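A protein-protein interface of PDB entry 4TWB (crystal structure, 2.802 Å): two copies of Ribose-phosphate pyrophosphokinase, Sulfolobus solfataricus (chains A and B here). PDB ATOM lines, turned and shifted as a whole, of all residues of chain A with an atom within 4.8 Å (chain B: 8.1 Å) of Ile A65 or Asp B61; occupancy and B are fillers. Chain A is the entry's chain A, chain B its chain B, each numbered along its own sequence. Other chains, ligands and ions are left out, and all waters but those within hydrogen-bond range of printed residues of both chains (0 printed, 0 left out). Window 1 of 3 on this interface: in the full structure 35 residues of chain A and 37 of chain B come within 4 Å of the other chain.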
ATOM      1  N   GLY A  35     -29.059   2.692  20.888  1.00  0.00           N
ATOM      2  CA  GLY A  35     -28.069   2.424  19.859  1.00  0.00           C
ATOM      3  C   GLY A  35     -27.002   1.481  20.405  1.00  0.00           C
ATOM      4  O   GLY A  35     -26.255   0.849  19.650  1.00  0.00           O
ATOM      5  N   SER A  37     -25.024  -1.623  22.512  1.00  0.00           N
ATOM      6  CA  SER A  37     -25.049  -3.065  22.354  1.00  0.00           C
ATOM      7  C   SER A  37     -25.307  -3.786  23.659  1.00  0.00           C
ATOM      8  O   SER A  37     -24.765  -3.414  24.701  1.00  0.00           O
ATOM      9  CB  SER A  37     -23.745  -3.559  21.737  1.00  0.00           C
ATOM     10  OG  SER A  37     -23.771  -3.399  20.334  1.00  0.00           O
ATOM     11  N   ASP A  61     -16.920  -0.290  14.073  1.00  0.00           N
ATOM     12  CA  ASP A  61     -16.785   0.238  15.416  1.00  0.00           C
ATOM     13  C   ASP A  61     -17.645  -0.526  16.412  1.00  0.00           C
ATOM     14  O   ASP A  61     -17.168  -0.938  17.486  1.00  0.00           O
ATOM     15  CB  ASP A  61     -17.079   1.729  15.425  1.00  0.00           C
ATOM     16  CG  ASP A  61     -16.197   2.483  14.453  1.00  0.00           C
ATOM     17  OD1 ASP A  61     -14.959   2.322  14.529  1.00  0.00           O
ATOM     18  OD2 ASP A  61     -16.735   3.212  13.595  1.00  0.00           O
ATOM     19  N   LYS A  62     -18.905  -0.739  16.055  1.00  0.00           N
ATOM     20  CA  LYS A  62     -19.775  -1.545  16.906  1.00  0.00           C
ATOM     21  C   LYS A  62     -19.235  -2.969  17.072  1.00  0.00           C
ATOM     22  O   LYS A  62     -19.180  -3.491  18.187  1.00  0.00           O
ATOM     23  CB  LYS A  62     -21.216  -1.572  16.391  1.00  0.00           C
ATOM     24  CG  LYS A  62     -22.114  -2.535  17.157  1.00  0.00           C
ATOM     25  CD  LYS A  62     -23.612  -2.325  16.860  1.00  0.00           C
ATOM     26  CE  LYS A  62     -24.154  -1.023  17.485  1.00  0.00           C
ATOM     27  NZ  LYS A  62     -24.134  -0.964  18.999  1.00  0.00           N
ATOM     28  N   HIS A  63     -18.825  -3.593  15.976  1.00  0.00           N
ATOM     29  CA  HIS A  63     -18.318  -4.955  16.065  1.00  0.00           C
ATOM     30  C   HIS A  63     -17.065  -5.025  16.936  1.00  0.00           C
ATOM     31  O   HIS A  63     -16.862  -5.993  17.661  1.00  0.00           O
ATOM     32  CB  HIS A  63     -18.069  -5.546  14.683  1.00  0.00           C
ATOM     33  CG  HIS A  63     -19.324  -5.909  13.968  1.00  0.00           C
ATOM     34  ND1 HIS A  63     -19.454  -5.821  12.598  1.00  0.00           N
ATOM     35  CD2 HIS A  63     -20.520  -6.345  14.437  1.00  0.00           C
ATOM     36  CE1 HIS A  63     -20.673  -6.200  12.253  1.00  0.00           C
ATOM     37  NE2 HIS A  63     -21.342  -6.520  13.350  1.00  0.00           N
ATOM     38  N   LEU A  64     -16.237  -3.989  16.882  1.00  0.00           N
ATOM     39  CA  LEU A  64     -15.044  -3.956  17.707  1.00  0.00           C
ATOM     40  C   LEU A  64     -15.413  -3.818  19.184  1.00  0.00           C
ATOM     41  O   LEU A  64     -14.832  -4.481  20.048  1.00  0.00           O
ATOM     42  CB  LEU A  64     -14.139  -2.801  17.293  1.00  0.00           C
ATOM     43  CG  LEU A  64     -13.179  -3.092  16.159  1.00  0.00           C
ATOM     44  CD1 LEU A  64     -12.576  -1.788  15.678  1.00  0.00           C
ATOM     45  CD2 LEU A  64     -12.112  -4.040  16.645  1.00  0.00           C
ATOM     46  N   ILE A  65     -16.371  -2.945  19.473  1.00  0.00           N
ATOM     47  CA  ILE A  65     -16.729  -2.728  20.858  1.00  0.00           C
ATOM     48  C   ILE A  65     -17.422  -3.968  21.387  1.00  0.00           C
ATOM     49  O   ILE A  65     -17.176  -4.386  22.519  1.00  0.00           O
ATOM     50  CB  ILE A  65     -17.502  -1.402  21.068  1.00  0.00           C
ATOM     51  CG1 ILE A  65     -16.482  -0.305  21.372  1.00  0.00           C
ATOM     52  CG2 ILE A  65     -18.466  -1.500  22.244  1.00  0.00           C
ATOM     53  CD1 ILE A  65     -16.945   1.058  21.033  1.00  0.00           C
ATOM     54  N   GLU A  66     -18.242  -4.593  20.547  1.00  0.00           N
ATOM     55  CA  GLU A  66     -18.844  -5.878  20.900  1.00  0.00           C
ATOM     56  C   GLU A  66     -17.776  -6.927  21.160  1.00  0.00           C
ATOM     57  O   GLU A  66     -17.871  -7.703  22.097  1.00  0.00           O
ATOM     58  CB  GLU A  66     -19.827  -6.340  19.829  1.00  0.00           C
ATOM     59  CG  GLU A  66     -21.207  -5.681  19.971  1.00  0.00           C
ATOM     60  CD  GLU A  66     -22.079  -5.844  18.739  1.00  0.00           C
ATOM     61  OE1 GLU A  66     -23.274  -5.479  18.793  1.00  0.00           O
ATOM     62  OE2 GLU A  66     -21.572  -6.336  17.712  1.00  0.00           O
ATOM     63  N   LEU A  67     -16.736  -6.933  20.341  1.00  0.00           N
ATOM     64  CA  LEU A  67     -15.622  -7.849  20.565  1.00  0.00           C
ATOM     65  C   LEU A  67     -15.001  -7.603  21.929  1.00  0.00           C
ATOM     66  O   LEU A  67     -14.827  -8.544  22.698  1.00  0.00           O
ATOM     67  CB  LEU A  67     -14.573  -7.738  19.446  1.00  0.00           C
ATOM     68  CG  LEU A  67     -13.236  -8.470  19.612  1.00  0.00           C
ATOM     69  CD1 LEU A  67     -13.420  -9.965  19.692  1.00  0.00           C
ATOM     70  CD2 LEU A  67     -12.318  -8.124  18.474  1.00  0.00           C
ATOM     71  N   PHE A  68     -14.674  -6.346  22.227  1.00  0.00           N
ATOM     72  CA  PHE A  68     -14.096  -5.988  23.523  1.00  0.00           C
ATOM     73  C   PHE A  68     -14.970  -6.462  24.677  1.00  0.00           C
ATOM     74  O   PHE A  68     -14.465  -7.036  25.644  1.00  0.00           O
ATOM     75  CB  PHE A  68     -13.901  -4.483  23.664  1.00  0.00           C
ATOM     76  CG  PHE A  68     -13.104  -3.867  22.571  1.00  0.00           C
ATOM     77  CD1 PHE A  68     -12.113  -4.574  21.932  1.00  0.00           C
ATOM     78  CD2 PHE A  68     -13.334  -2.556  22.197  1.00  0.00           C
ATOM     79  CE1 PHE A  68     -11.369  -3.997  20.928  1.00  0.00           C
ATOM     80  CE2 PHE A  68     -12.598  -1.971  21.195  1.00  0.00           C
ATOM     81  CZ  PHE A  68     -11.608  -2.698  20.556  1.00  0.00           C
ATOM     82  N   LEU A  69     -16.275  -6.212  24.577  1.00  0.00           N
ATOM     83  CA  LEU A  69     -17.215  -6.560  25.646  1.00  0.00           C
ATOM     84  C   LEU A  69     -17.317  -8.067  25.855  1.00  0.00           C
ATOM     85  O   LEU A  69     -17.253  -8.545  26.995  1.00  0.00           O
ATOM     86  CB  LEU A  69     -18.600  -6.030  25.325  1.00  0.00           C
ATOM     87  CG  LEU A  69     -18.730  -4.519  25.264  1.00  0.00           C
ATOM     88  CD1 LEU A  69     -20.193  -4.144  25.046  1.00  0.00           C
ATOM     89  CD2 LEU A  69     -18.175  -3.900  26.541  1.00  0.00           C
ATOM     90  N   SER B  37     -12.859   5.413  10.854  1.00  0.00           N
ATOM     91  CA  SER B  37     -12.527   6.765  11.271  1.00  0.00           C
ATOM     92  C   SER B  37     -11.077   7.146  10.976  1.00  0.00           C
ATOM     93  O   SER B  37     -10.141   6.355  11.200  1.00  0.00           O
ATOM     94  CB  SER B  37     -12.815   6.949  12.768  1.00  0.00           C
ATOM     95  OG  SER B  37     -14.197   7.168  13.018  1.00  0.00           O
ATOM     96  N   THR B  56     -19.612  10.927  24.087  1.00  0.00           N
ATOM     97  CA  THR B  56     -19.847   9.655  23.425  1.00  0.00           C
ATOM     98  C   THR B  56     -21.326   9.376  23.181  1.00  0.00           C
ATOM     99  O   THR B  56     -21.752   8.219  23.198  1.00  0.00           O
ATOM    100  CB  THR B  56     -19.165   8.469  24.164  1.00  0.00           C
ATOM    101  OG1 THR B  56     -19.725   8.320  25.480  1.00  0.00           O
ATOM    102  CG2 THR B  56     -17.656   8.689  24.254  1.00  0.00           C
ATOM    103  N   ASP B  57     -22.096  10.434  22.929  1.00  0.00           N
ATOM    104  CA  ASP B  57     -23.464  10.279  22.408  1.00  0.00           C
ATOM    105  C   ASP B  57     -23.522   9.564  21.045  1.00  0.00           C
ATOM    106  O   ASP B  57     -22.488   9.192  20.491  1.00  0.00           O
ATOM    107  CB  ASP B  57     -24.193  11.630  22.333  1.00  0.00           C
ATOM    108  CG  ASP B  57     -23.521  12.638  21.377  1.00  0.00           C
ATOM    109  OD1 ASP B  57     -24.211  13.581  20.919  1.00  0.00           O
ATOM    110  OD2 ASP B  57     -22.319  12.510  21.093  1.00  0.00           O
ATOM    111  N   TYR B  58     -24.726   9.375  20.509  1.00  0.00           N
ATOM    112  CA  TYR B  58     -24.892   8.648  19.242  1.00  0.00           C
ATOM    113  C   TYR B  58     -24.121   9.294  18.096  1.00  0.00           C
ATOM    114  O   TYR B  58     -24.250  10.506  17.883  1.00  0.00           O
ATOM    115  CB  TYR B  58     -26.374   8.500  18.845  1.00  0.00           C
ATOM    116  CG  TYR B  58     -26.568   7.665  17.598  1.00  0.00           C
ATOM    117  CD1 TYR B  58     -26.771   6.288  17.676  1.00  0.00           C
ATOM    118  CD2 TYR B  58     -26.512   8.247  16.338  1.00  0.00           C
ATOM    119  CE1 TYR B  58     -26.939   5.527  16.539  1.00  0.00           C
ATOM    120  CE2 TYR B  58     -26.672   7.490  15.196  1.00  0.00           C
ATOM    121  CZ  TYR B  58     -26.885   6.131  15.304  1.00  0.00           C
ATOM    122  OH  TYR B  58     -27.037   5.378  14.162  1.00  0.00           O
ATOM    123  N   PRO B  59     -23.324   8.490  17.355  1.00  0.00           N
ATOM    124  CA  PRO B  59     -23.104   7.038  17.501  1.00  0.00           C
ATOM    125  C   PRO B  59     -22.071   6.668  18.573  1.00  0.00           C
ATOM    126  O   PRO B  59     -20.877   7.007  18.435  1.00  0.00           O
ATOM    127  CB  PRO B  59     -22.533   6.617  16.127  1.00  0.00           C
ATOM    128  CG  PRO B  59     -22.467   7.861  15.294  1.00  0.00           C
ATOM    129  CD  PRO B  59     -22.546   9.029  16.234  1.00  0.00           C
ATOM    130  N   GLN B  60     -22.518   5.933  19.594  1.00  0.00           N
ATOM    131  CA  GLN B  60     -21.673   5.637  20.761  1.00  0.00           C
ATOM    132  C   GLN B  60     -20.401   4.838  20.406  1.00  0.00           C
ATOM    133  O   GLN B  60     -19.289   5.147  20.863  1.00  0.00           O
ATOM    134  CB  GLN B  60     -22.475   4.938  21.869  1.00  0.00           C
ATOM    135  CG  GLN B  60     -23.717   5.702  22.326  1.00  0.00           C
ATOM    136  CD  GLN B  60     -24.893   5.480  21.410  1.00  0.00           C
ATOM    137  OE1 GLN B  60     -24.738   5.369  20.180  1.00  0.00           O
ATOM    138  NE2 GLN B  60     -26.081   5.390  21.997  1.00  0.00           N
ATOM    139  N   ASP B  61     -20.561   3.823  19.570  1.00  0.00           N
ATOM    140  CA  ASP B  61     -19.438   2.939  19.295  1.00  0.00           C
ATOM    141  C   ASP B  61     -18.330   3.642  18.536  1.00  0.00           C
ATOM    142  O   ASP B  61     -17.151   3.543  18.923  1.00  0.00           O
ATOM    143  CB  ASP B  61     -19.917   1.689  18.586  1.00  0.00           C
ATOM    144  CG  ASP B  61     -21.019   1.010  19.345  1.00  0.00           C
ATOM    145  OD1 ASP B  61     -20.796   0.731  20.538  1.00  0.00           O
ATOM    146  OD2 ASP B  61     -22.109   0.783  18.778  1.00  0.00           O
ATOM    147  N   LYS B  62     -18.695   4.360  17.468  1.00  0.00           N
ATOM    148  CA  LYS B  62     -17.708   5.149  16.737  1.00  0.00           C
ATOM    149  C   LYS B  62     -17.075   6.222  17.625  1.00  0.00           C
ATOM    150  O   LYS B  62     -15.859   6.412  17.605  1.00  0.00           O
ATOM    151  CB  LYS B  62     -18.307   5.780  15.485  1.00  0.00           C
ATOM    152  CG  LYS B  62     -17.371   6.795  14.802  1.00  0.00           C
ATOM    153  CD  LYS B  62     -17.843   7.165  13.390  1.00  0.00           C
ATOM    154  CE  LYS B  62     -17.710   5.979  12.403  1.00  0.00           C
ATOM    155  NZ  LYS B  62     -16.310   5.464  12.144  1.00  0.00           N
ATOM    156  N   HIS B  63     -17.886   6.915  18.425  1.00  0.00           N
ATOM    157  CA  HIS B  63     -17.331   7.970  19.256  1.00  0.00           C
ATOM    158  C   HIS B  63     -16.396   7.400  20.307  1.00  0.00           C
ATOM    159  O   HIS B  63     -15.386   8.012  20.654  1.00  0.00           O
ATOM    160  CB  HIS B  63     -18.426   8.801  19.886  1.00  0.00           C
ATOM    161  CG  HIS B  63     -19.073   9.756  18.940  1.00  0.00           C
ATOM    162  ND1 HIS B  63     -20.407  10.083  19.012  1.00  0.00           N
ATOM    163  CD2 HIS B  63     -18.569  10.456  17.900  1.00  0.00           C
ATOM    164  CE1 HIS B  63     -20.700  10.942  18.052  1.00  0.00           C
ATOM    165  NE2 HIS B  63     -19.601  11.184  17.363  1.00  0.00           N
ATOM    166  N   LEU B  64     -16.723   6.210  20.800  1.00  0.00           N
ATOM    167  CA  LEU B  64     -15.849   5.528  21.748  1.00  0.00           C
ATOM    168  C   LEU B  64     -14.532   5.159  21.100  1.00  0.00           C
ATOM    169  O   LEU B  64     -13.470   5.400  21.670  1.00  0.00           O
ATOM    170  CB  LEU B  64     -16.524   4.288  22.308  1.00  0.00           C
ATOM    171  CG  LEU B  64     -17.445   4.587  23.487  1.00  0.00           C
ATOM    172  CD1 LEU B  64     -18.307   3.367  23.775  1.00  0.00           C
ATOM    173  CD2 LEU B  64     -16.635   5.009  24.708  1.00  0.00           C
ATOM    174  N   ILE B  65     -14.600   4.572  19.905  1.00  0.00           N
ATOM    175  CA  ILE B  65     -13.383   4.117  19.249  1.00  0.00           C
ATOM    176  C   ILE B  65     -12.545   5.321  18.858  1.00  0.00           C
ATOM    177  O   ILE B  65     -11.332   5.336  19.077  1.00  0.00           O
ATOM    178  CB  ILE B  65     -13.666   3.138  18.093  1.00  0.00           C
ATOM    179  CG1 ILE B  65     -13.645   1.717  18.647  1.00  0.00           C
ATOM    180  CG2 ILE B  65     -12.599   3.247  17.018  1.00  0.00           C
ATOM    181  CD1 ILE B  65     -14.417   0.733  17.858  1.00  0.00           C
ATOM    182  N   GLU B  66     -13.196   6.360  18.347  1.00  0.00           N
ATOM    183  CA  GLU B  66     -12.506   7.626  18.124  1.00  0.00           C
ATOM    184  C   GLU B  66     -11.827   8.158  19.399  1.00  0.00           C
ATOM    185  O   GLU B  66     -10.688   8.629  19.353  1.00  0.00           O
ATOM    186  CB  GLU B  66     -13.469   8.651  17.548  1.00  0.00           C
ATOM    187  CG  GLU B  66     -13.633   8.517  16.031  1.00  0.00           C
ATOM    188  CD  GLU B  66     -14.846   9.265  15.487  1.00  0.00           C
ATOM    189  OE1 GLU B  66     -15.042   9.269  14.249  1.00  0.00           O
ATOM    190  OE2 GLU B  66     -15.597   9.846  16.296  1.00  0.00           O
ATOM    191  N   LEU B  67     -12.522   8.063  20.536  1.00  0.00           N
ATOM    192  CA  LEU B  67     -11.938   8.448  21.823  1.00  0.00           C
ATOM    193  C   LEU B  67     -10.678   7.654  22.099  1.00  0.00           C
ATOM    194  O   LEU B  67      -9.639   8.239  22.401  1.00  0.00           O
ATOM    195  CB  LEU B  67     -12.945   8.301  22.982  1.00  0.00           C
ATOM    196  CG  LEU B  67     -12.438   8.453  24.431  1.00  0.00           C
ATOM    197  CD1 LEU B  67     -11.894   9.853  24.707  1.00  0.00           C
ATOM    198  CD2 LEU B  67     -13.562   8.122  25.359  1.00  0.00           C
ATOM    199  N   PHE B  68     -10.769   6.334  21.979  1.00  0.00           N
ATOM    200  CA  PHE B  68      -9.612   5.469  22.203  1.00  0.00           C
ATOM    201  C   PHE B  68      -8.431   5.884  21.327  1.00  0.00           C
ATOM    202  O   PHE B  68      -7.289   5.944  21.799  1.00  0.00           O
ATOM    203  CB  PHE B  68      -9.939   4.002  21.913  1.00  0.00           C
ATOM    204  CG  PHE B  68     -11.118   3.474  22.666  1.00  0.00           C
ATOM    205  CD1 PHE B  68     -11.424   3.957  23.920  1.00  0.00           C
ATOM    206  CD2 PHE B  68     -11.908   2.483  22.123  1.00  0.00           C
ATOM    207  CE1 PHE B  68     -12.510   3.477  24.612  1.00  0.00           C
ATOM    208  CE2 PHE B  68     -12.989   1.995  22.815  1.00  0.00           C
ATOM    209  CZ  PHE B  68     -13.291   2.492  24.062  1.00  0.00           C
ATOM    210  N   ALA B  90     -20.930   6.703  27.440  1.00  0.00           N
ATOM    211  CA  ALA B  90     -21.839   5.657  26.933  1.00  0.00           C
ATOM    212  C   ALA B  90     -21.684   4.345  27.721  1.00  0.00           C
ATOM    213  O   ALA B  90     -20.705   4.161  28.447  1.00  0.00           O
ATOM    214  CB  ALA B  90     -21.651   5.430  25.418  1.00  0.00           C
ATOM    215  N   TYR B  91     -22.661   3.453  27.579  1.00  0.00           N
ATOM    216  CA  TYR B  91     -22.641   2.171  28.282  1.00  0.00           C
ATOM    217  C   TYR B  91     -22.680   2.351  29.803  1.00  0.00           C
ATOM    218  O   TYR B  91     -22.203   1.504  30.552  1.00  0.00           O
ATOM    219  CB  TYR B  91     -21.468   1.293  27.803  1.00  0.00           C
ATOM    220  CG  TYR B  91     -21.675   0.828  26.369  1.00  0.00           C
ATOM    221  CD1 TYR B  91     -22.372  -0.331  26.098  1.00  0.00           C
ATOM    222  CD2 TYR B  91     -21.227   1.587  25.294  1.00  0.00           C
ATOM    223  CE1 TYR B  91     -22.595  -0.734  24.814  1.00  0.00           C
ATOM    224  CE2 TYR B  91     -21.451   1.190  24.010  1.00  0.00           C
ATOM    225  CZ  TYR B  91     -22.136   0.032  23.776  1.00  0.00           C
ATOM    226  OH  TYR B  91     -22.368  -0.380  22.493  1.00  0.00           O
ATOM    227  N   ALA B 103     -22.532  -8.818  30.038  1.00  0.00           N
ATOM    228  CA  ALA B 103     -21.312  -8.032  30.100  1.00  0.00           C
ATOM    229  C   ALA B 103     -21.501  -6.835  31.009  1.00  0.00           C
ATOM    230  O   ALA B 103     -22.544  -6.183  31.015  1.00  0.00           O
ATOM    231  CB  ALA B 103     -20.923  -7.561  28.721  1.00  0.00           C
ATOM    232  N   SER B 105     -20.559  -3.729  30.634  1.00  0.00           N
ATOM    233  CA  SER B 105     -20.020  -2.865  29.578  1.00  0.00           C
ATOM    234  C   SER B 105     -19.169  -1.718  30.124  1.00  0.00           C
ATOM    235  O   SER B 105     -18.084  -1.423  29.612  1.00  0.00           O
ATOM    236  CB  SER B 105     -21.144  -2.305  28.708  1.00  0.00           C
ATOM    237  OG  SER B 105     -22.056  -3.320  28.299  1.00  0.00           O
ATOM    238  N   THR B 108     -15.509  -2.605  31.013  1.00  0.00           N
ATOM    239  CA  THR B 108     -14.647  -2.741  29.851  1.00  0.00           C
ATOM    240  C   THR B 108     -14.249  -1.381  29.303  1.00  0.00           C
ATOM    241  O   THR B 108     -13.079  -1.114  29.043  1.00  0.00           O
ATOM    242  CB  THR B 108     -15.364  -3.517  28.732  1.00  0.00           C
ATOM    243  OG1 THR B 108     -15.776  -4.812  29.207  1.00  0.00           O
ATOM    244  CG2 THR B 108     -14.441  -3.677  27.567  1.00  0.00           C
ATOM    245  N   ILE B 109     -15.237  -0.521  29.117  1.00  0.00           N
ATOM    246  CA  ILE B 109     -14.982   0.800  28.575  1.00  0.00           C
ATOM    247  C   ILE B 109     -13.988   1.537  29.451  1.00  0.00           C
ATOM    248  O   ILE B 109     -13.030   2.145  28.954  1.00  0.00           O
ATOM    249  CB  ILE B 109     -16.254   1.644  28.535  1.00  0.00           C
ATOM    250  CG1 ILE B 109     -17.324   0.992  27.657  1.00  0.00           C
ATOM    251  CG2 ILE B 109     -15.930   3.022  28.038  1.00  0.00           C
ATOM    252  CD1 ILE B 109     -16.989   1.022  26.186  1.00  0.00           C
ATOM    253  N   ILE B 112     -10.481   0.139  29.415  1.00  0.00           N
ATOM    254  CA  ILE B 112      -9.886   0.507  28.133  1.00  0.00           C
ATOM    255  C   ILE B 112      -9.331   1.925  28.177  1.00  0.00           C
ATOM    256  O   ILE B 112      -8.343   2.219  27.520  1.00  0.00           O
ATOM    257  CB  ILE B 112     -10.902   0.399  26.969  1.00  0.00           C
ATOM    258  CG1 ILE B 112     -11.161  -1.053  26.606  1.00  0.00           C
ATOM    259  CG2 ILE B 112     -10.414   1.125  25.740  1.00  0.00           C
ATOM    260  CD1 ILE B 112     -12.009  -1.224  25.366  1.00  0.00           C
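The side-chain amino group of Lys A62 lies within salt-bridge range of the side-chain carboxylate of Asp B61.
The side-chain hydroxyl (OH) of Tyr B91 sits at hydrogen-bond distance from the backbone NH (N) of Ser A37 (2.9 Å).
The side-chain carboxylate of Asp A61 lies within salt-bridge range of the side-chain amino group of Lys B62.
The side-chain hydroxyl (OG) of Ser A37 lies within hydrogen-bond range of the side-chain carboxylate (OE1) of Glu A66 (2.6 Å).
OD1 of Asp B61 is in hydrogen-bond range of OH of Tyr B91.
OG of Ser B37 is in hydrogen-bond range of NZ of Lys B62 (2.9 Å).
The backbone carbonyl oxygen of Gly A35 sits at hydrogen-bond distance from the side-chain amino group of Lys A62 (2.9 Å).
OG of Ser A37 is in hydrogen-bond range of NZ of Lys A62, 2.8 Å away.
Asp A61 touches Asp B61.
Ile B65 touches Asp A61 (CD1 to O, 3.2 Å).
Lys A62 touches Tyr B91 (NZ to OH, 3.96 Å).
CB of Leu A64 touches CD1 of Ile B65 (3.6 Å).
Ile A65 touches Asp B61 (CD1 to O, 3.3 Å).
Leu B64 touches Ile A65 (CB to CD1, 3.5 Å).
Thr B108 touches Phe A68.
Phe A68 touches Ile B112 (CD2 to CD1, 3.7 Å).
Leu A69 touches Ser B105 (CD2 to CA, 3.7 Å).
CB of Thr B108 touches CD2 of Leu A69, at 3.6 Å.
Of chain B, only Asp B61 (3.3 Å) and Leu B64 (3.5 Å) come within 4 Å of Ile A65.
Asp B61 touches three residues of chain A.
Lys A62 touches two residues of chain B.
Printed residues of chain A within 4 Å of Thr B108: Phe A68 and Leu A69.
Printed residues of chain B within 4 Å of Leu A69: Ser B105 (3.7 Å) and Thr B108 (3.6 Å).
Printed residues of chain B within 4 Å of Ser A37: Tyr B91.
The nearest residue of chain A that does not touch Asp B61 is Gly A35 (4.2 Å).
Of the 21 printed residues of chain B, 8 touch a printed residue of chain A.
Printed residues of chain B that touch a printed residue of chain A: Asp B61, Lys B62, Leu B64, Ile B65, Tyr B91, Ser B105, Thr B108 and Ile B112.
Hydrophobic or aromatic side chains of chain B within 4 Å of the printed part of chain A: Leu B64, Ile B65, Tyr B91 and Ile B112.
Printed residues of chain A that touch a printed residue of chain B: Ser A37, Asp A61, Lys A62, Leu A64, Ile A65, Phe A68 and Leu A69.
Along chain A the printed residues that touch a printed residue of chain B span positions 37 to 69.
Among the printed residues, 13 pairs touch across the chains.
Asp B61 touches its own counterpart, Asp A61.
Asp A61 touches Lys B62, and with the chains exchanged Lys A62 touches Asp B61.
Asp A61 touches Ile B65, and with the chains exchanged Ile A65 touches Asp B61.
Leu A64 touches Ile B65, and with the chains exchanged Ile A65 touches Leu B64.
9 positions are printed for both chains.
Of the 13 pairs that touch across the chains among the printed residues, 7 have their exchanged pair printed and touching as well.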
